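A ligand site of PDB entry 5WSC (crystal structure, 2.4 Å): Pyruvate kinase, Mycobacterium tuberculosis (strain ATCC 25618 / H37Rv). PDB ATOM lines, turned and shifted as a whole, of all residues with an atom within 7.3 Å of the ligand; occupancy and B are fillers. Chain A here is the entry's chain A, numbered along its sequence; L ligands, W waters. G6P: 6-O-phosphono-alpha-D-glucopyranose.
ND1 of His 348 is in hydrogen-bond range of OE2 of Glu 270 (2.6 Å).
OG1 of Thr 352 sits at hydrogen-bond distance from N of Gly 355 (2.9 Å).
The side-chain amide nitrogen of Asn 271 is in hydrogen-bond range of the backbone carbonyl oxygen of Met 267 (3.1 Å).
The guanidinium group (NE) of Arg 388 sits at hydrogen-bond distance from the backbone carbonyl oxygen (O) of Arg 385.
The backbone carbonyl oxygen of Gly 355 sits at hydrogen-bond distance from the side-chain hydroxyl of Ser 358 (3.0 Å).
The backbone carbonyl oxygen (O) of Leu 236 is in hydrogen-bond range of the side-chain amino group (NZ) of Lys 273.
NZ of Lys 273 sits at hydrogen-bond distance from O of Val 235, 2.7 Å away.
N of Lys 273 lies within hydrogen-bond range of O of Ala 268 (3.0 Å).
An oxygen (O3P) of the ligand lies within hydrogen-bond range of a ring nitrogen (NE2) of His 348 (2.5 Å).
An oxygen (O2P) of the ligand is in hydrogen-bond range of the backbone NH (N) of Arg 351 (2.7 Å).
N of Thr 352 is in hydrogen-bond range of O2P of the ligand.
An oxygen (O1P) of the ligand lies within hydrogen-bond range of the side-chain hydroxyl (OG1) of Thr 352 (2.9 Å).
O of Asn 271 lies within hydrogen-bond range of O1 of the ligand (3.0 Å).
OD1 of Asn 271 sits close to O5 of the ligand (3.3 Å).
The guanidinium group (NH1) of Arg 385 lies within salt-bridge range of an oxygen (O1P) of the ligand (3.1 Å).
O3P of the ligand is in salt-bridge range of NH1 of Arg 388.
CD2 of Leu 236 touches O2 of the ligand (3.7 Å).
Glu 270 touches the ligand.
Lys 273 touches the ligand.
Pro 350 touches the ligand.
CA of Gly 355 touches O1P of the ligand (3.6 Å).
11 residues have an atom within 4 Å of the ligand: Leu 236, Glu 270, Asn 271, Lys 273, His 348, Pro 350, Arg 351, Thr 352, Gly 355, Arg 385 and Arg 388.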
ATOM      1  N   VAL A 235       1.959 -19.346   0.777  1.00  0.00           N
ATOM      2  CA  VAL A 235       0.839 -18.649   0.218  1.00  0.00           C
ATOM      3  C   VAL A 235       1.262 -17.381  -0.525  1.00  0.00           C
ATOM      4  O   VAL A 235       0.652 -17.034  -1.542  1.00  0.00           O
ATOM      5  CB  VAL A 235      -0.161 -18.237   1.314  1.00  0.00           C
ATOM      6  CG1 VAL A 235      -1.209 -17.241   0.788  1.00  0.00           C
ATOM      7  CG2 VAL A 235      -0.841 -19.481   1.898  1.00  0.00           C
ATOM      8  N   LEU A 236       2.267 -16.674  -0.016  1.00  0.00           N
ATOM      9  CA  LEU A 236       2.715 -15.402  -0.634  1.00  0.00           C
ATOM     10  C   LEU A 236       3.617 -15.644  -1.851  1.00  0.00           C
ATOM     11  O   LEU A 236       3.577 -14.871  -2.807  1.00  0.00           O
ATOM     12  CB  LEU A 236       3.447 -14.524   0.383  1.00  0.00           C
ATOM     13  CG  LEU A 236       2.604 -13.811   1.449  1.00  0.00           C
ATOM     14  CD1 LEU A 236       3.440 -13.418   2.656  1.00  0.00           C
ATOM     15  CD2 LEU A 236       1.958 -12.595   0.842  1.00  0.00           C
ATOM     16  N   MET A 267      -5.787 -18.289   5.273  1.00  0.00           N
ATOM     17  CA  MET A 267      -4.534 -17.600   4.919  1.00  0.00           C
ATOM     18  C   MET A 267      -4.536 -17.283   3.382  1.00  0.00           C
ATOM     19  O   MET A 267      -4.138 -16.206   2.928  1.00  0.00           O
ATOM     20  CB  MET A 267      -3.368 -18.461   5.343  1.00  0.00           C
ATOM     21  CG  MET A 267      -1.973 -17.843   5.166  1.00  0.00           C
ATOM     22  SD  MET A 267      -1.693 -16.399   6.225  1.00  0.00           S
ATOM     23  CE  MET A 267      -1.356 -17.210   7.798  1.00  0.00           C
ATOM     24  N   ALA A 268      -5.078 -18.203   2.594  1.00  0.00           N
ATOM     25  CA  ALA A 268      -5.322 -17.922   1.213  1.00  0.00           C
ATOM     26  C   ALA A 268      -6.237 -16.700   1.059  1.00  0.00           C
ATOM     27  O   ALA A 268      -5.884 -15.763   0.390  1.00  0.00           O
ATOM     28  CB  ALA A 268      -5.928 -19.133   0.548  1.00  0.00           C
ATOM     29  N   ARG A 269      -7.401 -16.688   1.676  1.00  0.00           N
ATOM     30  CA  ARG A 269      -8.299 -15.552   1.512  1.00  0.00           C
ATOM     31  C   ARG A 269      -7.703 -14.230   2.035  1.00  0.00           C
ATOM     32  O   ARG A 269      -8.036 -13.170   1.531  1.00  0.00           O
ATOM     33  CB  ARG A 269      -9.620 -15.806   2.205  1.00  0.00           C
ATOM     34  CG  ARG A 269     -10.458 -16.859   1.570  1.00  0.00           C
ATOM     35  CD  ARG A 269     -11.684 -17.142   2.407  1.00  0.00           C
ATOM     36  NE  ARG A 269     -12.440 -15.925   2.579  1.00  0.00           N
ATOM     37  CZ  ARG A 269     -12.774 -15.376   3.752  1.00  0.00           C
ATOM     38  NH1 ARG A 269     -12.437 -15.940   4.924  1.00  0.00           N
ATOM     39  NH2 ARG A 269     -13.442 -14.221   3.749  1.00  0.00           N
ATOM     40  N   GLU A 270      -6.868 -14.282   3.072  1.00  0.00           N
ATOM     41  CA  GLU A 270      -6.308 -13.065   3.656  1.00  0.00           C
ATOM     42  C   GLU A 270      -5.421 -12.396   2.599  1.00  0.00           C
ATOM     43  O   GLU A 270      -5.349 -11.156   2.521  1.00  0.00           O
ATOM     44  CB  GLU A 270      -5.433 -13.360   4.885  1.00  0.00           C
ATOM     45  CG  GLU A 270      -6.155 -13.789   6.173  1.00  0.00           C
ATOM     46  CD  GLU A 270      -6.879 -12.667   6.888  1.00  0.00           C
ATOM     47  OE1 GLU A 270      -7.713 -13.007   7.760  1.00  0.00           O
ATOM     48  OE2 GLU A 270      -6.624 -11.462   6.596  1.00  0.00           O
ATOM     49  N   ASN A 271      -4.740 -13.213   1.804  1.00  0.00           N
ATOM     50  CA  ASN A 271      -3.799 -12.693   0.825  1.00  0.00           C
ATOM     51  C   ASN A 271      -4.335 -12.805  -0.605  1.00  0.00           C
ATOM     52  O   ASN A 271      -3.573 -12.620  -1.572  1.00  0.00           O
ATOM     53  CB  ASN A 271      -2.470 -13.426   0.943  1.00  0.00           C
ATOM     54  CG  ASN A 271      -1.788 -13.189   2.282  1.00  0.00           C
ATOM     55  OD1 ASN A 271      -1.309 -12.088   2.579  1.00  0.00           O
ATOM     56  ND2 ASN A 271      -1.720 -14.202   3.069  1.00  0.00           N
ATOM     57  N   ALA A 272      -5.629 -13.135  -0.744  1.00  0.00           N
ATOM     58  CA  ALA A 272      -6.300 -13.144  -2.033  1.00  0.00           C
ATOM     59  C   ALA A 272      -5.716 -14.152  -3.028  1.00  0.00           C
ATOM     60  O   ALA A 272      -5.500 -13.832  -4.216  1.00  0.00           O
ATOM     61  CB  ALA A 272      -6.284 -11.752  -2.612  1.00  0.00           C
ATOM     62  N   LYS A 273      -5.454 -15.351  -2.547  1.00  0.00           N
ATOM     63  CA  LYS A 273      -4.948 -16.436  -3.378  1.00  0.00           C
ATOM     64  C   LYS A 273      -5.982 -17.511  -3.355  1.00  0.00           C
ATOM     65  O   LYS A 273      -6.523 -17.817  -2.317  1.00  0.00           O
ATOM     66  CB  LYS A 273      -3.640 -16.992  -2.789  1.00  0.00           C
ATOM     67  CG  LYS A 273      -2.550 -15.934  -2.550  1.00  0.00           C
ATOM     68  CD  LYS A 273      -2.227 -15.137  -3.803  1.00  0.00           C
ATOM     69  CE  LYS A 273      -1.003 -14.255  -3.593  1.00  0.00           C
ATOM     70  NZ  LYS A 273       0.191 -15.116  -3.438  1.00  0.00           N
ATOM     71  N   LEU A 346     -12.226 -11.504   7.309  1.00  0.00           N
ATOM     72  CA  LEU A 346     -10.784 -11.287   7.250  1.00  0.00           C
ATOM     73  C   LEU A 346     -10.312 -10.636   8.561  1.00  0.00           C
ATOM     74  O   LEU A 346     -11.044  -9.859   9.169  1.00  0.00           O
ATOM     75  CB  LEU A 346     -10.438 -10.384   6.065  1.00  0.00           C
ATOM     76  CG  LEU A 346     -10.865 -10.898   4.685  1.00  0.00           C
ATOM     77  CD1 LEU A 346     -10.368  -9.925   3.605  1.00  0.00           C
ATOM     78  CD2 LEU A 346     -10.295 -12.268   4.402  1.00  0.00           C
ATOM     79  N   HIS A 348      -7.763  -8.572   8.877  1.00  0.00           N
ATOM     80  CA  HIS A 348      -7.301  -7.194   8.673  1.00  0.00           C
ATOM     81  C   HIS A 348      -8.213  -6.398   7.761  1.00  0.00           C
ATOM     82  O   HIS A 348      -8.981  -6.964   6.984  1.00  0.00           O
ATOM     83  CB  HIS A 348      -5.885  -7.156   8.081  1.00  0.00           C
ATOM     84  CG  HIS A 348      -5.800  -7.719   6.691  1.00  0.00           C
ATOM     85  ND1 HIS A 348      -5.611  -9.060   6.451  1.00  0.00           N
ATOM     86  CD2 HIS A 348      -5.903  -7.133   5.476  1.00  0.00           C
ATOM     87  CE1 HIS A 348      -5.573  -9.270   5.142  1.00  0.00           C
ATOM     88  NE2 HIS A 348      -5.752  -8.114   4.537  1.00  0.00           N
ATOM     89  N   ILE A 349      -8.137  -5.070   7.893  1.00  0.00           N
ATOM     90  CA  ILE A 349      -8.695  -4.125   6.941  1.00  0.00           C
ATOM     91  C   ILE A 349      -7.822  -4.165   5.693  1.00  0.00           C
ATOM     92  O   ILE A 349      -6.620  -4.062   5.803  1.00  0.00           O
ATOM     93  CB  ILE A 349      -8.650  -2.668   7.480  1.00  0.00           C
ATOM     94  CG1 ILE A 349      -9.288  -2.564   8.875  1.00  0.00           C
ATOM     95  CG2 ILE A 349      -9.350  -1.705   6.525  1.00  0.00           C
ATOM     96  CD1 ILE A 349     -10.593  -3.328   8.995  1.00  0.00           C
ATOM     97  N   PRO A 350      -8.410  -4.321   4.499  1.00  0.00           N
ATOM     98  CA  PRO A 350      -7.596  -4.298   3.279  1.00  0.00           C
ATOM     99  C   PRO A 350      -6.812  -2.972   3.102  1.00  0.00           C
ATOM    100  O   PRO A 350      -7.355  -1.876   3.366  1.00  0.00           O
ATOM    101  CB  PRO A 350      -8.616  -4.446   2.165  1.00  0.00           C
ATOM    102  CG  PRO A 350      -9.785  -5.125   2.797  1.00  0.00           C
ATOM    103  CD  PRO A 350      -9.807  -4.707   4.235  1.00  0.00           C
ATOM    104  N   ARG A 351      -5.567  -3.095   2.659  1.00  0.00           N
ATOM    105  CA  ARG A 351      -4.601  -1.964   2.670  1.00  0.00           C
ATOM    106  C   ARG A 351      -4.059  -1.640   1.248  1.00  0.00           C
ATOM    107  O   ARG A 351      -3.610  -0.527   0.990  1.00  0.00           O
ATOM    108  CB  ARG A 351      -3.430  -2.335   3.574  1.00  0.00           C
ATOM    109  CG  ARG A 351      -2.435  -1.197   3.788  1.00  0.00           C
ATOM    110  CD  ARG A 351      -1.676  -1.353   5.121  1.00  0.00           C
ATOM    111  NE  ARG A 351      -2.520  -1.407   6.335  1.00  0.00           N
ATOM    112  CZ  ARG A 351      -2.776  -0.376   7.159  1.00  0.00           C
ATOM    113  NH1 ARG A 351      -2.298   0.854   6.909  1.00  0.00           N
ATOM    114  NH2 ARG A 351      -3.536  -0.555   8.237  1.00  0.00           N
ATOM    115  N   THR A 352      -4.074  -2.630   0.346  1.00  0.00           N
ATOM    116  CA  THR A 352      -3.682  -2.406  -1.040  1.00  0.00           C
ATOM    117  C   THR A 352      -4.804  -1.718  -1.777  1.00  0.00           C
ATOM    118  O   THR A 352      -5.998  -1.920  -1.502  1.00  0.00           O
ATOM    119  CB  THR A 352      -3.410  -3.716  -1.811  1.00  0.00           C
ATOM    120  OG1 THR A 352      -4.643  -4.431  -2.020  1.00  0.00           O
ATOM    121  CG2 THR A 352      -2.400  -4.561  -1.089  1.00  0.00           C
ATOM    122  N   LYS A 353      -4.423  -0.896  -2.739  1.00  0.00           N
ATOM    123  CA  LYS A 353      -5.397  -0.217  -3.567  1.00  0.00           C
ATOM    124  C   LYS A 353      -6.473  -1.182  -4.082  1.00  0.00           C
ATOM    125  O   LYS A 353      -7.642  -0.928  -3.945  1.00  0.00           O
ATOM    126  CB  LYS A 353      -4.676   0.429  -4.756  1.00  0.00           C
ATOM    127  CG  LYS A 353      -5.549   1.381  -5.524  1.00  0.00           C
ATOM    128  CD  LYS A 353      -4.730   2.233  -6.475  1.00  0.00           C
ATOM    129  CE  LYS A 353      -3.939   1.410  -7.495  1.00  0.00           C
ATOM    130  NZ  LYS A 353      -3.914   2.111  -8.808  1.00  0.00           N
ATOM    131  N   ARG A 354      -6.051  -2.291  -4.651  1.00  0.00           N
ATOM    132  CA  ARG A 354      -6.968  -3.196  -5.293  1.00  0.00           C
ATOM    133  C   ARG A 354      -7.882  -3.871  -4.318  1.00  0.00           C
ATOM    134  O   ARG A 354      -9.049  -4.162  -4.629  1.00  0.00           O
ATOM    135  CB  ARG A 354      -6.212  -4.240  -6.114  1.00  0.00           C
ATOM    136  CG  ARG A 354      -5.858  -3.722  -7.485  1.00  0.00           C
ATOM    137  CD  ARG A 354      -5.003  -4.732  -8.201  1.00  0.00           C
ATOM    138  NE  ARG A 354      -3.676  -4.828  -7.609  1.00  0.00           N
ATOM    139  CZ  ARG A 354      -2.701  -5.553  -8.138  1.00  0.00           C
ATOM    140  NH1 ARG A 354      -2.914  -6.211  -9.262  1.00  0.00           N
ATOM    141  NH2 ARG A 354      -1.527  -5.620  -7.568  1.00  0.00           N
ATOM    142  N   GLY A 355      -7.356  -4.106  -3.116  1.00  0.00           N
ATOM    143  CA  GLY A 355      -8.136  -4.668  -2.054  1.00  0.00           C
ATOM    144  C   GLY A 355      -9.110  -3.662  -1.465  1.00  0.00           C
ATOM    145  O   GLY A 355     -10.261  -4.013  -1.178  1.00  0.00           O
ATOM    146  N   VAL A 356      -8.654  -2.412  -1.297  1.00  0.00           N
ATOM    147  CA  VAL A 356      -9.501  -1.368  -0.718  1.00  0.00           C
ATOM    148  C   VAL A 356     -10.641  -1.060  -1.676  1.00  0.00           C
ATOM    149  O   VAL A 356     -11.792  -0.943  -1.254  1.00  0.00           O
ATOM    150  CB  VAL A 356      -8.728  -0.064  -0.481  1.00  0.00           C
ATOM    151  CG1 VAL A 356      -9.675   1.108  -0.214  1.00  0.00           C
ATOM    152  CG2 VAL A 356      -7.769  -0.188   0.655  1.00  0.00           C
ATOM    153  N   SER A 358     -11.771  -3.012  -4.251  1.00  0.00           N
ATOM    154  CA  SER A 358     -12.663  -4.157  -4.376  1.00  0.00           C
ATOM    155  C   SER A 358     -13.583  -4.251  -3.157  1.00  0.00           C
ATOM    156  O   SER A 358     -14.762  -4.411  -3.276  1.00  0.00           O
ATOM    157  CB  SER A 358     -11.890  -5.461  -4.592  1.00  0.00           C
ATOM    158  OG  SER A 358     -10.904  -5.653  -3.621  1.00  0.00           O
ATOM    159  N   ASP A 381      -6.068 -10.280 -10.246  1.00  0.00           N
ATOM    160  CA  ASP A 381      -5.858  -9.926  -8.821  1.00  0.00           C
ATOM    161  C   ASP A 381      -7.034  -9.157  -8.271  1.00  0.00           C
ATOM    162  O   ASP A 381      -7.612  -9.527  -7.265  1.00  0.00           O
ATOM    163  CB  ASP A 381      -4.565  -9.129  -8.668  1.00  0.00           C
ATOM    164  CG  ASP A 381      -4.337  -8.675  -7.244  1.00  0.00           C
ATOM    165  OD1 ASP A 381      -4.944  -7.642  -6.874  1.00  0.00           O
ATOM    166  OD2 ASP A 381      -3.607  -9.376  -6.472  1.00  0.00           O
ATOM    167  N   ARG A 385      -9.532 -10.309  -5.012  1.00  0.00           N
ATOM    168  CA  ARG A 385      -9.703  -9.566  -3.791  1.00  0.00           C
ATOM    169  C   ARG A 385     -11.146  -9.296  -3.493  1.00  0.00           C
ATOM    170  O   ARG A 385     -11.508  -9.069  -2.344  1.00  0.00           O
ATOM    171  CB  ARG A 385      -8.924  -8.258  -3.835  1.00  0.00           C
ATOM    172  CG  ARG A 385      -7.470  -8.505  -4.101  1.00  0.00           C
ATOM    173  CD  ARG A 385      -6.592  -7.354  -3.660  1.00  0.00           C
ATOM    174  NE  ARG A 385      -5.254  -7.734  -4.029  1.00  0.00           N
ATOM    175  CZ  ARG A 385      -4.365  -8.291  -3.219  1.00  0.00           C
ATOM    176  NH1 ARG A 385      -4.640  -8.416  -1.939  1.00  0.00           N
ATOM    177  NH2 ARG A 385      -3.184  -8.676  -3.712  1.00  0.00           N
ATOM    178  N   ARG A 388     -12.819 -13.215  -2.598  1.00  0.00           N
ATOM    179  CA  ARG A 388     -12.521 -13.695  -1.257  1.00  0.00           C
ATOM    180  C   ARG A 388     -13.502 -13.163  -0.230  1.00  0.00           C
ATOM    181  O   ARG A 388     -13.615 -13.733   0.863  1.00  0.00           O
ATOM    182  CB  ARG A 388     -11.124 -13.281  -0.841  1.00  0.00           C
ATOM    183  CG  ARG A 388     -11.007 -11.806  -0.490  1.00  0.00           C
ATOM    184  CD  ARG A 388      -9.576 -11.357  -0.316  1.00  0.00           C
ATOM    185  NE  ARG A 388      -9.490  -9.891  -0.289  1.00  0.00           N
ATOM    186  CZ  ARG A 388      -8.478  -9.183   0.233  1.00  0.00           C
ATOM    187  NH1 ARG A 388      -7.428  -9.780   0.800  1.00  0.00           N
ATOM    188  NH2 ARG A 388      -8.530  -7.844   0.210  1.00  0.00           N
HETATM  189  C1  G6P L   1      -1.147  -9.751  -1.070  1.00  0.00           C
HETATM  190  C2  G6P L   1       0.221  -9.059  -1.057  1.00  0.00           C
HETATM  191  C3  G6P L   1       0.580  -8.562   0.306  1.00  0.00           C
HETATM  192  C4  G6P L   1      -0.602  -7.962   0.994  1.00  0.00           C
HETATM  193  C5  G6P L   1      -1.662  -8.978   1.255  1.00  0.00           C
HETATM  194  C6  G6P L   1      -2.950  -8.320   1.722  1.00  0.00           C
HETATM  195  O1  G6P L   1      -1.018 -11.081  -1.522  1.00  0.00           O
HETATM  196  O2  G6P L   1       1.285  -9.888  -1.539  1.00  0.00           O
HETATM  197  O3  G6P L   1       1.550  -7.538   0.144  1.00  0.00           O
HETATM  198  O4  G6P L   1      -0.161  -7.559   2.277  1.00  0.00           O
HETATM  199  O5  G6P L   1      -1.876  -9.868   0.158  1.00  0.00           O
HETATM  200  O6  G6P L   1      -3.464  -7.435   0.741  1.00  0.00           O
HETATM  201  P   G6P L   1      -4.760  -6.601   1.223  1.00  0.00           P
HETATM  202  O1P G6P L   1      -5.590  -6.203   0.042  1.00  0.00           O
HETATM  203  O2P G6P L   1      -4.267  -5.405   2.017  1.00  0.00           O
HETATM  204  O3P G6P L   1      -5.534  -7.587   2.061  1.00  0.00           O
HETATM  205  O   HOH W   1       4.036  -8.826   0.024  1.00  0.00           O
